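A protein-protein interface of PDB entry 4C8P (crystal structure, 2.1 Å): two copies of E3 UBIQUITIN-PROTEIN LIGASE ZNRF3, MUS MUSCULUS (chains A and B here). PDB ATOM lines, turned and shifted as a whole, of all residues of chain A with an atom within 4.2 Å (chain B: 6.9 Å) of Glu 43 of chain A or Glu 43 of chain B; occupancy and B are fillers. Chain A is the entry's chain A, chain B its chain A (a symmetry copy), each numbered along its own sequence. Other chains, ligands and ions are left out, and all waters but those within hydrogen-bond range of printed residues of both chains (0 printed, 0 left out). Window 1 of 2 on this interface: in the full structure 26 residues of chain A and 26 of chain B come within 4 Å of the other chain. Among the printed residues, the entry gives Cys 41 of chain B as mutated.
Of the 19 printed residues of chain B, 10 touch a printed residue of chain A.
Hydrophobic or aromatic side chains of chain B that line the printed part of chain A: Tyr 66.
Of the 10 printed residues of chain A, 8 touch a printed residue of chain B.
Among the printed residues, 22 pairs touch across the chains.
Among the printed residues, Asp or Glu carboxylates within 4 Å of a Lys or Arg side-chain nitrogen of the other chain: Glu 43 of chain A with Arg 126 of chain B and Arg 126 of chain A with Glu 43 of chain B.
Ala 42 of chain A touches Glu 43 of chain B, and with the chains exchanged Glu 43 of chain A touches Ala 42 of chain B.
Glu 43 of chain A touches Thr 100 of chain B, and with the chains exchanged Thr 100 of chain A touches Glu 43 of chain B.
Glu 43 of chain A touches Arg 150 of chain B, and with the chains exchanged Arg 150 of chain A touches Glu 43 of chain B.
Gly 44 of chain A touches Arg 150 of chain B, and with the chains exchanged Arg 150 of chain A touches Gly 44 of chain B.
10 positions are printed for both chains.
Of the 22 pairs that touch across the chains among the printed residues, 18 have their exchanged pair printed and touching as well.
Among the printed residues, merely in contact across the chains: Ala 42 of chain A with Glu 43 of chain B, Glu 43 of chain A with Ala 42 of chain B, Arg 150 of chain A with Gly 44 of chain B, Gly 44 of chain A with Arg 150 of chain B, Arg 150 of chain A with Tyr 66 of chain B, Arg 152 of chain A with Tyr 66 of chain B and Arg 152 of chain A with Cys 41 of chain B.
The backbone carbonyl oxygen (O) of Gly 98 of chain B is in hydrogen-bond range of the backbone NH (N) of Gly 67 of chain B.
The guanidinium group (NE) of Arg 150 of chain B lies within salt-bridge range of the side-chain carboxylate (OE2) of Glu 43 of chain B (2.8 Å).
The backbone carbonyl oxygen (O) of Thr 100 of chain A is in hydrogen-bond range of the guanidinium group (NE) of Arg 126 of chain A (2.9 Å).
The guanidinium group (NE) of Arg 152 of chain B is in salt-bridge range of the side-chain carboxylate (OE1) of Glu 43 of chain B.
The backbone NH (N) of Gly 44 of chain A sits at hydrogen-bond distance from the backbone carbonyl oxygen (O) of Ala 151 of chain A, at 2.9 Å.
The backbone NH (N) of Thr 100 of chain B sits at hydrogen-bond distance from the backbone carbonyl oxygen (O) of Trp 68 of chain B (2.8 Å).
The guanidinium group (NH2) of Arg 150 of chain A sits at hydrogen-bond distance from the backbone carbonyl oxygen (O) of Glu 43 of chain B (2.8 Å).
The guanidinium group of Arg 126 of chain B lies within salt-bridge range of the side-chain carboxylate of Glu 43 of chain A, 3.7 Å away.
The backbone carbonyl oxygen (O) of Gly 67 of chain A sits at hydrogen-bond distance from the guanidinium group (NH2) of Arg 150 of chain B, 3.3 Å away.
The guanidinium group of Arg 150 of chain A sits close to the guanidinium group of Arg 150 of chain B (3.5 Å).
OG1 of Thr 100 of chain A sits at hydrogen-bond distance from NH2 of Arg 152 of chain B (3.2 Å).
NH2 of Arg 126 of chain B sits close to NE of Arg 152 of chain A (3.3 Å).
OG1 of Thr 100 of chain B is in hydrogen-bond range of NH2 of Arg 152 of chain A (3.2 Å).
The backbone NH (N) of Ala 42 of chain A is in hydrogen-bond range of the side-chain sulfur (SG) of Cys 41 of chain B (3.8 Å).
The backbone carbonyl oxygen (O) of Gly 67 of chain B sits at hydrogen-bond distance from the guanidinium group (NH2) of Arg 150 of chain A (3.3 Å).
N of Glu 43 of chain A sits at hydrogen-bond distance from OE1 of Glu 43 of chain B (3.1 Å).
OG1 of Thr 100 of chain A is in hydrogen-bond range of OE2 of Glu 43 of chain B, at 2.9 Å.
The side-chain hydroxyl (OG1) of Thr 100 of chain B is in hydrogen-bond range of the side-chain carboxylate (OE2) of Glu 43 of chain A.
The backbone carbonyl oxygen (O) of Glu 43 of chain A lies within hydrogen-bond range of the guanidinium group (NH2) of Arg 150 of chain B, 2.8 Å away.
The guanidinium group (NH2) of Arg 126 of chain A sits close to the guanidinium group (NE) of Arg 152 of chain B (3.3 Å).
NH2 of Arg 126 of chain A is in salt-bridge range of OE1 of Glu 43 of chain B (3.7 Å).
Of the printed residues of chain A, Ala 42 of chain B touches Glu 43 (3.4 Å).
Of chain A, only Ala 42, Glu 43, Thr 100, Arg 126 and Arg 150 come within 4 Å of Glu 43 of chain B.
Of the printed residues of chain A, Gly 67 of chain B touches Arg 150.
Val 69 of chain B touches none of the printed residues of chain A.
Of the printed residues of chain A, Thr 100 of chain B touches Glu 43 and Arg 152.
Of the printed residues of chain A, Arg 126 of chain B touches Glu 43 (3.7 Å) and Arg 152 (3.3 Å).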
ATOM      1  N   ALA A  42      -9.405  -8.242   8.387  1.00  0.00           N
ATOM      2  CA  ALA A  42      -9.651  -9.396   9.234  1.00  0.00           C
ATOM      3  C   ALA A  42     -11.083  -9.866   9.067  1.00  0.00           C
ATOM      4  O   ALA A  42     -11.972  -9.051   8.815  1.00  0.00           O
ATOM      5  CB  ALA A  42      -9.370  -9.046  10.686  1.00  0.00           C
ATOM      6  N   GLU A  43     -11.304 -11.184   9.203  1.00  0.00           N
ATOM      7  CA  GLU A  43     -12.657 -11.704   9.108  1.00  0.00           C
ATOM      8  C   GLU A  43     -12.742 -12.989   9.918  1.00  0.00           C
ATOM      9  O   GLU A  43     -11.794 -13.793   9.895  1.00  0.00           O
ATOM     10  CB  GLU A  43     -13.086 -11.974   7.638  1.00  0.00           C
ATOM     11  CG  GLU A  43     -14.556 -12.406   7.474  1.00  0.00           C
ATOM     12  CD  GLU A  43     -14.889 -12.876   6.053  1.00  0.00           C
ATOM     13  OE1 GLU A  43     -14.259 -12.344   5.106  1.00  0.00           O
ATOM     14  OE2 GLU A  43     -15.770 -13.789   5.871  1.00  0.00           O
ATOM     15  N   GLY A  44     -13.825 -13.152  10.675  1.00  0.00           N
ATOM     16  CA  GLY A  44     -13.965 -14.417  11.444  1.00  0.00           C
ATOM     17  C   GLY A  44     -15.204 -14.418  12.264  1.00  0.00           C
ATOM     18  O   GLY A  44     -15.874 -13.393  12.417  1.00  0.00           O
ATOM     19  N   GLY A  67      -8.801 -18.039  14.514  1.00  0.00           N
ATOM     20  CA  GLY A  67      -9.292 -17.066  13.557  1.00  0.00           C
ATOM     21  C   GLY A  67     -10.551 -16.332  13.944  1.00  0.00           C
ATOM     22  O   GLY A  67     -11.146 -15.667  13.109  1.00  0.00           O
ATOM     23  N   VAL A  69     -12.912 -13.372  15.858  1.00  0.00           N
ATOM     24  CA  VAL A  69     -12.845 -11.984  16.122  1.00  0.00           C
ATOM     25  C   VAL A  69     -13.407 -11.717  17.514  1.00  0.00           C
ATOM     26  O   VAL A  69     -14.597 -11.808  17.697  1.00  0.00           O
ATOM     27  CB  VAL A  69     -13.651 -11.190  15.062  1.00  0.00           C
ATOM     28  CG1 VAL A  69     -13.684  -9.716  15.450  1.00  0.00           C
ATOM     29  CG2 VAL A  69     -13.034 -11.396  13.684  1.00  0.00           C
ATOM     30  N   THR A 100      -8.035 -13.222  15.199  1.00  0.00           N
ATOM     31  CA  THR A 100      -7.533 -12.578  14.001  1.00  0.00           C
ATOM     32  C   THR A 100      -7.705 -11.011  14.112  1.00  0.00           C
ATOM     33  O   THR A 100      -7.053 -10.228  13.436  1.00  0.00           O
ATOM     34  CB  THR A 100      -8.224 -13.165  12.739  1.00  0.00           C
ATOM     35  OG1 THR A 100      -7.688 -12.557  11.555  1.00  0.00           O
ATOM     36  CG2 THR A 100      -9.706 -12.910  12.727  1.00  0.00           C
ATOM     37  N   ARG A 126      -2.107  -8.097  13.991  1.00  0.00           N
ATOM     38  CA  ARG A 126      -3.546  -8.196  13.650  1.00  0.00           C
ATOM     39  C   ARG A 126      -4.228  -6.909  14.091  1.00  0.00           C
ATOM     40  O   ARG A 126      -3.691  -6.189  14.939  1.00  0.00           O
ATOM     41  CB  ARG A 126      -4.148  -9.391  14.393  1.00  0.00           C
ATOM     42  CG  ARG A 126      -3.470 -10.736  14.068  1.00  0.00           C
ATOM     43  CD  ARG A 126      -3.364 -10.980  12.546  1.00  0.00           C
ATOM     44  NE  ARG A 126      -4.682 -10.829  11.919  1.00  0.00           N
ATOM     45  CZ  ARG A 126      -4.929 -10.430  10.668  1.00  0.00           C
ATOM     46  NH1 ARG A 126      -3.960 -10.130   9.859  1.00  0.00           N
ATOM     47  NH2 ARG A 126      -6.184 -10.280  10.241  1.00  0.00           N
ATOM     48  N   ARG A 150     -20.618 -13.244  12.173  1.00  0.00           N
ATOM     49  CA  ARG A 150     -19.325 -13.152  11.597  1.00  0.00           C
ATOM     50  C   ARG A 150     -18.940 -11.653  11.360  1.00  0.00           C
ATOM     51  O   ARG A 150     -19.712 -10.822  10.849  1.00  0.00           O
ATOM     52  CB  ARG A 150     -19.281 -13.999  10.304  1.00  0.00           C
ATOM     53  CG  ARG A 150     -17.875 -14.304   9.814  1.00  0.00           C
ATOM     54  CD  ARG A 150     -17.833 -15.113   8.533  1.00  0.00           C
ATOM     55  NE  ARG A 150     -16.454 -15.354   8.056  1.00  0.00           N
ATOM     56  CZ  ARG A 150     -15.668 -16.324   8.506  1.00  0.00           C
ATOM     57  NH1 ARG A 150     -16.115 -17.139   9.445  1.00  0.00           N
ATOM     58  NH2 ARG A 150     -14.450 -16.514   8.009  1.00  0.00           N
ATOM     59  N   ALA A 151     -17.738 -11.297  11.774  1.00  0.00           N
ATOM     60  CA  ALA A 151     -17.312  -9.959  11.615  1.00  0.00           C
ATOM     61  C   ALA A 151     -16.308  -9.957  10.481  1.00  0.00           C
ATOM     62  O   ALA A 151     -15.576 -10.921  10.289  1.00  0.00           O
ATOM     63  CB  ALA A 151     -16.695  -9.439  12.893  1.00  0.00           C
ATOM     64  N   ARG A 152     -16.339  -8.873   9.731  1.00  0.00           N
ATOM     65  CA  ARG A 152     -15.389  -8.586   8.659  1.00  0.00           C
ATOM     66  C   ARG A 152     -14.958  -7.139   8.870  1.00  0.00           C
ATOM     67  O   ARG A 152     -15.824  -6.255   8.973  1.00  0.00           O
ATOM     68  CB  ARG A 152     -16.076  -8.750   7.319  1.00  0.00           C
ATOM     69  CG  ARG A 152     -15.166  -8.738   6.109  1.00  0.00           C
ATOM     70  CD  ARG A 152     -15.987  -8.997   4.863  1.00  0.00           C
ATOM     71  NE  ARG A 152     -16.427 -10.392   4.809  1.00  0.00           N
ATOM     72  CZ  ARG A 152     -17.683 -10.820   4.743  1.00  0.00           C
ATOM     73  NH1 ARG A 152     -18.711  -9.975   4.714  1.00  0.00           N
ATOM     74  NH2 ARG A 152     -17.911 -12.133   4.693  1.00  0.00           N
ATOM     75  N   VAL B  12      -2.542 -19.754   6.311  1.00  0.00           N
ATOM     76  CA  VAL B  12      -2.121 -20.022   7.675  1.00  0.00           C
ATOM     77  C   VAL B  12      -2.415 -21.460   8.143  1.00  0.00           C
ATOM     78  O   VAL B  12      -3.557 -21.927   8.188  1.00  0.00           O
ATOM     79  CB  VAL B  12      -2.780 -19.021   8.629  1.00  0.00           C
ATOM     80  CG1 VAL B  12      -2.130 -19.065  10.012  1.00  0.00           C
ATOM     81  CG2 VAL B  12      -2.699 -17.612   8.022  1.00  0.00           C
ATOM     82  N   CYS B  41     -11.417  -7.352   1.042  1.00  0.00           N
ATOM     83  CA  CYS B  41     -10.922  -8.250   2.085  1.00  0.00           C
ATOM     84  C   CYS B  41     -11.774  -9.506   2.203  1.00  0.00           C
ATOM     85  O   CYS B  41     -13.020  -9.457   2.249  1.00  0.00           O
ATOM     86  CB  CYS B  41     -11.015  -7.568   3.498  1.00  0.00           C
ATOM     87  SG  CYS B  41     -11.053  -8.683   5.016  1.00  0.00           S
ATOM     88  N   ALA B  42     -11.090 -10.613   2.412  1.00  0.00           N
ATOM     89  CA  ALA B  42     -11.773 -11.843   2.773  1.00  0.00           C
ATOM     90  C   ALA B  42     -10.864 -12.713   3.619  1.00  0.00           C
ATOM     91  O   ALA B  42      -9.645 -12.682   3.443  1.00  0.00           O
ATOM     92  CB  ALA B  42     -12.207 -12.585   1.519  1.00  0.00           C
ATOM     93  N   GLU B  43     -11.460 -13.485   4.543  1.00  0.00           N
ATOM     94  CA  GLU B  43     -10.660 -14.385   5.357  1.00  0.00           C
ATOM     95  C   GLU B  43     -11.533 -15.552   5.791  1.00  0.00           C
ATOM     96  O   GLU B  43     -12.714 -15.348   6.117  1.00  0.00           O
ATOM     97  CB  GLU B  43     -10.061 -13.678   6.605  1.00  0.00           C
ATOM     98  CG  GLU B  43      -9.102 -14.555   7.434  1.00  0.00           C
ATOM     99  CD  GLU B  43      -8.702 -13.915   8.768  1.00  0.00           C
ATOM    100  OE1 GLU B  43      -8.635 -12.661   8.810  1.00  0.00           O
ATOM    101  OE2 GLU B  43      -8.467 -14.654   9.788  1.00  0.00           O
ATOM    102  N   GLY B  44     -10.987 -16.765   5.731  1.00  0.00           N
ATOM    103  CA  GLY B  44     -11.793 -17.927   6.191  1.00  0.00           C
ATOM    104  C   GLY B  44     -11.053 -19.203   6.019  1.00  0.00           C
ATOM    105  O   GLY B  44     -10.003 -19.255   5.372  1.00  0.00           O
ATOM    106  N   GLU B  45     -11.609 -20.268   6.609  1.00  0.00           N
ATOM    107  CA  GLU B  45     -11.060 -21.592   6.439  1.00  0.00           C
ATOM    108  C   GLU B  45     -11.101 -21.963   4.962  1.00  0.00           C
ATOM    109  O   GLU B  45     -12.126 -21.767   4.288  1.00  0.00           O
ATOM    110  CB  GLU B  45     -11.856 -22.632   7.280  1.00  0.00           C
ATOM    111  CG  GLU B  45     -11.117 -23.969   7.445  1.00  0.00           C
ATOM    112  CD  GLU B  45     -11.908 -25.054   8.201  1.00  0.00           C
ATOM    113  OE1 GLU B  45     -12.963 -24.743   8.797  1.00  0.00           O
ATOM    114  OE2 GLU B  45     -11.480 -26.242   8.193  1.00  0.00           O
ATOM    115  N   TYR B  66     -20.789 -21.166   7.011  1.00  0.00           N
ATOM    116  CA  TYR B  66     -20.705 -19.883   6.338  1.00  0.00           C
ATOM    117  C   TYR B  66     -19.277 -19.311   6.490  1.00  0.00           C
ATOM    118  O   TYR B  66     -18.697 -19.408   7.553  1.00  0.00           O
ATOM    119  CB  TYR B  66     -21.791 -18.903   6.851  1.00  0.00           C
ATOM    120  CG  TYR B  66     -21.740 -17.580   6.097  1.00  0.00           C
ATOM    121  CD1 TYR B  66     -22.302 -17.437   4.839  1.00  0.00           C
ATOM    122  CD2 TYR B  66     -21.062 -16.502   6.625  1.00  0.00           C
ATOM    123  CE1 TYR B  66     -22.206 -16.223   4.138  1.00  0.00           C
ATOM    124  CE2 TYR B  66     -20.932 -15.301   5.935  1.00  0.00           C
ATOM    125  CZ  TYR B  66     -21.499 -15.161   4.692  1.00  0.00           C
ATOM    126  OH  TYR B  66     -21.352 -13.935   4.063  1.00  0.00           O
ATOM    127  N   GLY B  67     -18.709 -18.793   5.396  1.00  0.00           N
ATOM    128  CA  GLY B  67     -17.517 -17.968   5.443  1.00  0.00           C
ATOM    129  C   GLY B  67     -16.233 -18.637   5.022  1.00  0.00           C
ATOM    130  O   GLY B  67     -15.163 -18.087   5.242  1.00  0.00           O
ATOM    131  N   TRP B  68     -16.349 -19.778   4.353  1.00  0.00           N
ATOM    132  CA  TRP B  68     -15.176 -20.475   3.815  1.00  0.00           C
ATOM    133  C   TRP B  68     -14.542 -19.773   2.604  1.00  0.00           C
ATOM    134  O   TRP B  68     -15.194 -19.072   1.911  1.00  0.00           O
ATOM    135  CB  TRP B  68     -15.492 -21.915   3.411  1.00  0.00           C
ATOM    136  CG  TRP B  68     -16.754 -22.119   2.599  1.00  0.00           C
ATOM    137  CD1 TRP B  68     -18.066 -22.117   3.069  1.00  0.00           C
ATOM    138  CD2 TRP B  68     -16.847 -22.439   1.199  1.00  0.00           C
ATOM    139  NE1 TRP B  68     -18.942 -22.392   2.034  1.00  0.00           N
ATOM    140  CE2 TRP B  68     -18.217 -22.575   0.879  1.00  0.00           C
ATOM    141  CE3 TRP B  68     -15.912 -22.659   0.194  1.00  0.00           C
ATOM    142  CZ2 TRP B  68     -18.651 -22.882  -0.414  1.00  0.00           C
ATOM    143  CZ3 TRP B  68     -16.364 -22.991  -1.073  1.00  0.00           C
ATOM    144  CH2 TRP B  68     -17.713 -23.096  -1.357  1.00  0.00           C
ATOM    145  N   VAL B  69     -13.280 -20.080   2.339  1.00  0.00           N
ATOM    146  CA  VAL B  69     -12.637 -19.651   1.154  1.00  0.00           C
ATOM    147  C   VAL B  69     -12.439 -20.852   0.236  1.00  0.00           C
ATOM    148  O   VAL B  69     -11.608 -21.680   0.519  1.00  0.00           O
ATOM    149  CB  VAL B  69     -11.268 -19.002   1.483  1.00  0.00           C
ATOM    150  CG1 VAL B  69     -10.535 -18.682   0.185  1.00  0.00           C
ATOM    151  CG2 VAL B  69     -11.478 -17.756   2.333  1.00  0.00           C
ATOM    152  N   GLY B  98     -22.172 -20.061   0.854  1.00  0.00           N
ATOM    153  CA  GLY B  98     -21.429 -19.580   2.018  1.00  0.00           C
ATOM    154  C   GLY B  98     -19.938 -19.190   1.871  1.00  0.00           C
ATOM    155  O   GLY B  98     -19.260 -18.894   2.869  1.00  0.00           O
ATOM    156  N   ALA B  99     -19.416 -19.181   0.662  1.00  0.00           N
ATOM    157  CA  ALA B  99     -18.030 -18.787   0.437  1.00  0.00           C
ATOM    158  C   ALA B  99     -17.898 -17.297   0.588  1.00  0.00           C
ATOM    159  O   ALA B  99     -18.735 -16.582   0.074  1.00  0.00           O
ATOM    160  CB  ALA B  99     -17.588 -19.204  -0.944  1.00  0.00           C
ATOM    161  N   THR B 100     -16.834 -16.842   1.281  1.00  0.00           N
ATOM    162  CA  THR B 100     -16.535 -15.432   1.438  1.00  0.00           C
ATOM    163  C   THR B 100     -15.563 -14.951   0.289  1.00  0.00           C
ATOM    164  O   THR B 100     -15.450 -13.775  -0.029  1.00  0.00           O
ATOM    165  CB  THR B 100     -15.963 -15.154   2.857  1.00  0.00           C
ATOM    166  OG1 THR B 100     -15.715 -13.750   3.021  1.00  0.00           O
ATOM    167  CG2 THR B 100     -14.658 -15.858   3.097  1.00  0.00           C
ATOM    168  N   ALA B 101     -14.946 -15.927  -0.348  1.00  0.00           N
ATOM    169  CA  ALA B 101     -13.934 -15.767  -1.356  1.00  0.00           C
ATOM    170  C   ALA B 101     -13.830 -17.066  -2.159  1.00  0.00           C
ATOM    171  O   ALA B 101     -14.129 -18.250  -1.643  1.00  0.00           O
ATOM    172  CB  ALA B 101     -12.612 -15.464  -0.686  1.00  0.00           C
ATOM    173  N   ARG B 126     -18.302 -10.541  -3.301  1.00  0.00           N
ATOM    174  CA  ARG B 126     -17.133 -11.134  -2.610  1.00  0.00           C
ATOM    175  C   ARG B 126     -16.010 -11.289  -3.625  1.00  0.00           C
ATOM    176  O   ARG B 126     -16.270 -11.300  -4.832  1.00  0.00           O
ATOM    177  CB  ARG B 126     -17.532 -12.503  -2.054  1.00  0.00           C
ATOM    178  CG  ARG B 126     -18.717 -12.458  -1.070  1.00  0.00           C
ATOM    179  CD  ARG B 126     -18.508 -11.406   0.043  1.00  0.00           C
ATOM    180  NE  ARG B 126     -17.216 -11.622   0.702  1.00  0.00           N
ATOM    181  CZ  ARG B 126     -16.450 -10.691   1.280  1.00  0.00           C
ATOM    182  NH1 ARG B 126     -16.816  -9.447   1.306  1.00  0.00           N
ATOM    183  NH2 ARG B 126     -15.263 -11.017   1.796  1.00  0.00           N
ATOM    184  N   ARG B 150      -6.133 -21.644   6.752  1.00  0.00           N
ATOM    185  CA  ARG B 150      -6.935 -20.475   6.689  1.00  0.00           C
ATOM    186  C   ARG B 150      -6.339 -19.463   5.653  1.00  0.00           C
ATOM    187  O   ARG B 150      -5.131 -19.175   5.597  1.00  0.00           O
ATOM    188  CB  ARG B 150      -7.076 -19.876   8.108  1.00  0.00           C
ATOM    189  CG  ARG B 150      -8.208 -18.873   8.243  1.00  0.00           C
ATOM    190  CD  ARG B 150      -8.330 -18.267   9.628  1.00  0.00           C
ATOM    191  NE  ARG B 150      -9.411 -17.261   9.717  1.00  0.00           N
ATOM    192  CZ  ARG B 150     -10.690 -17.556   9.908  1.00  0.00           C
ATOM    193  NH1 ARG B 150     -11.055 -18.820  10.023  1.00  0.00           N
ATOM    194  NH2 ARG B 150     -11.610 -16.604  10.018  1.00  0.00           N
ATOM    195  N   ALA B 151      -7.201 -18.946   4.797  1.00  0.00           N
ATOM    196  CA  ALA B 151      -6.749 -18.035   3.816  1.00  0.00           C
ATOM    197  C   ALA B 151      -7.216 -16.662   4.252  1.00  0.00           C
ATOM    198  O   ALA B 151      -8.270 -16.522   4.862  1.00  0.00           O
ATOM    199  CB  ALA B 151      -7.303 -18.394   2.457  1.00  0.00           C
ATOM    200  N   ARG B 152      -6.381 -15.685   3.959  1.00  0.00           N
ATOM    201  CA  ARG B 152      -6.666 -14.268   4.166  1.00  0.00           C
ATOM    202  C   ARG B 152      -6.261 -13.574   2.871  1.00  0.00           C
ATOM    203  O   ARG B 152      -5.122 -13.757   2.412  1.00  0.00           O
ATOM    204  CB  ARG B 152      -5.842 -13.753   5.328  1.00  0.00           C
ATOM    205  CG  ARG B 152      -6.209 -12.374   5.833  1.00  0.00           C
ATOM    206  CD  ARG B 152      -5.359 -12.041   7.042  1.00  0.00           C
ATOM    207  NE  ARG B 152      -5.771 -12.831   8.203  1.00  0.00           N
ATOM    208  CZ  ARG B 152      -5.006 -13.658   8.905  1.00  0.00           C
ATOM    209  NH1 ARG B 152      -3.723 -13.853   8.605  1.00  0.00           N
ATOM    210  NH2 ARG B 152      -5.541 -14.299   9.946  1.00  0.00           N
ATOM    211  N   ILE B 153      -7.211 -12.846   2.263  1.00  0.00           N
ATOM    212  CA  ILE B 153      -7.058 -12.195   0.942  1.00  0.00           C
ATOM    213  C   ILE B 153      -7.229 -10.690   1.145  1.00  0.00           C
ATOM    214  O   ILE B 153      -8.195 -10.281   1.816  1.00  0.00           O
ATOM    215  CB  ILE B 153      -8.174 -12.658  -0.025  1.00  0.00           C
ATOM    216  CG1 ILE B 153      -8.154 -14.185  -0.225  1.00  0.00           C
ATOM    217  CG2 ILE B 153      -8.140 -11.943  -1.382  1.00  0.00           C
ATOM    218  CD1 ILE B 153      -9.311 -14.634  -1.050  1.00  0.00           C
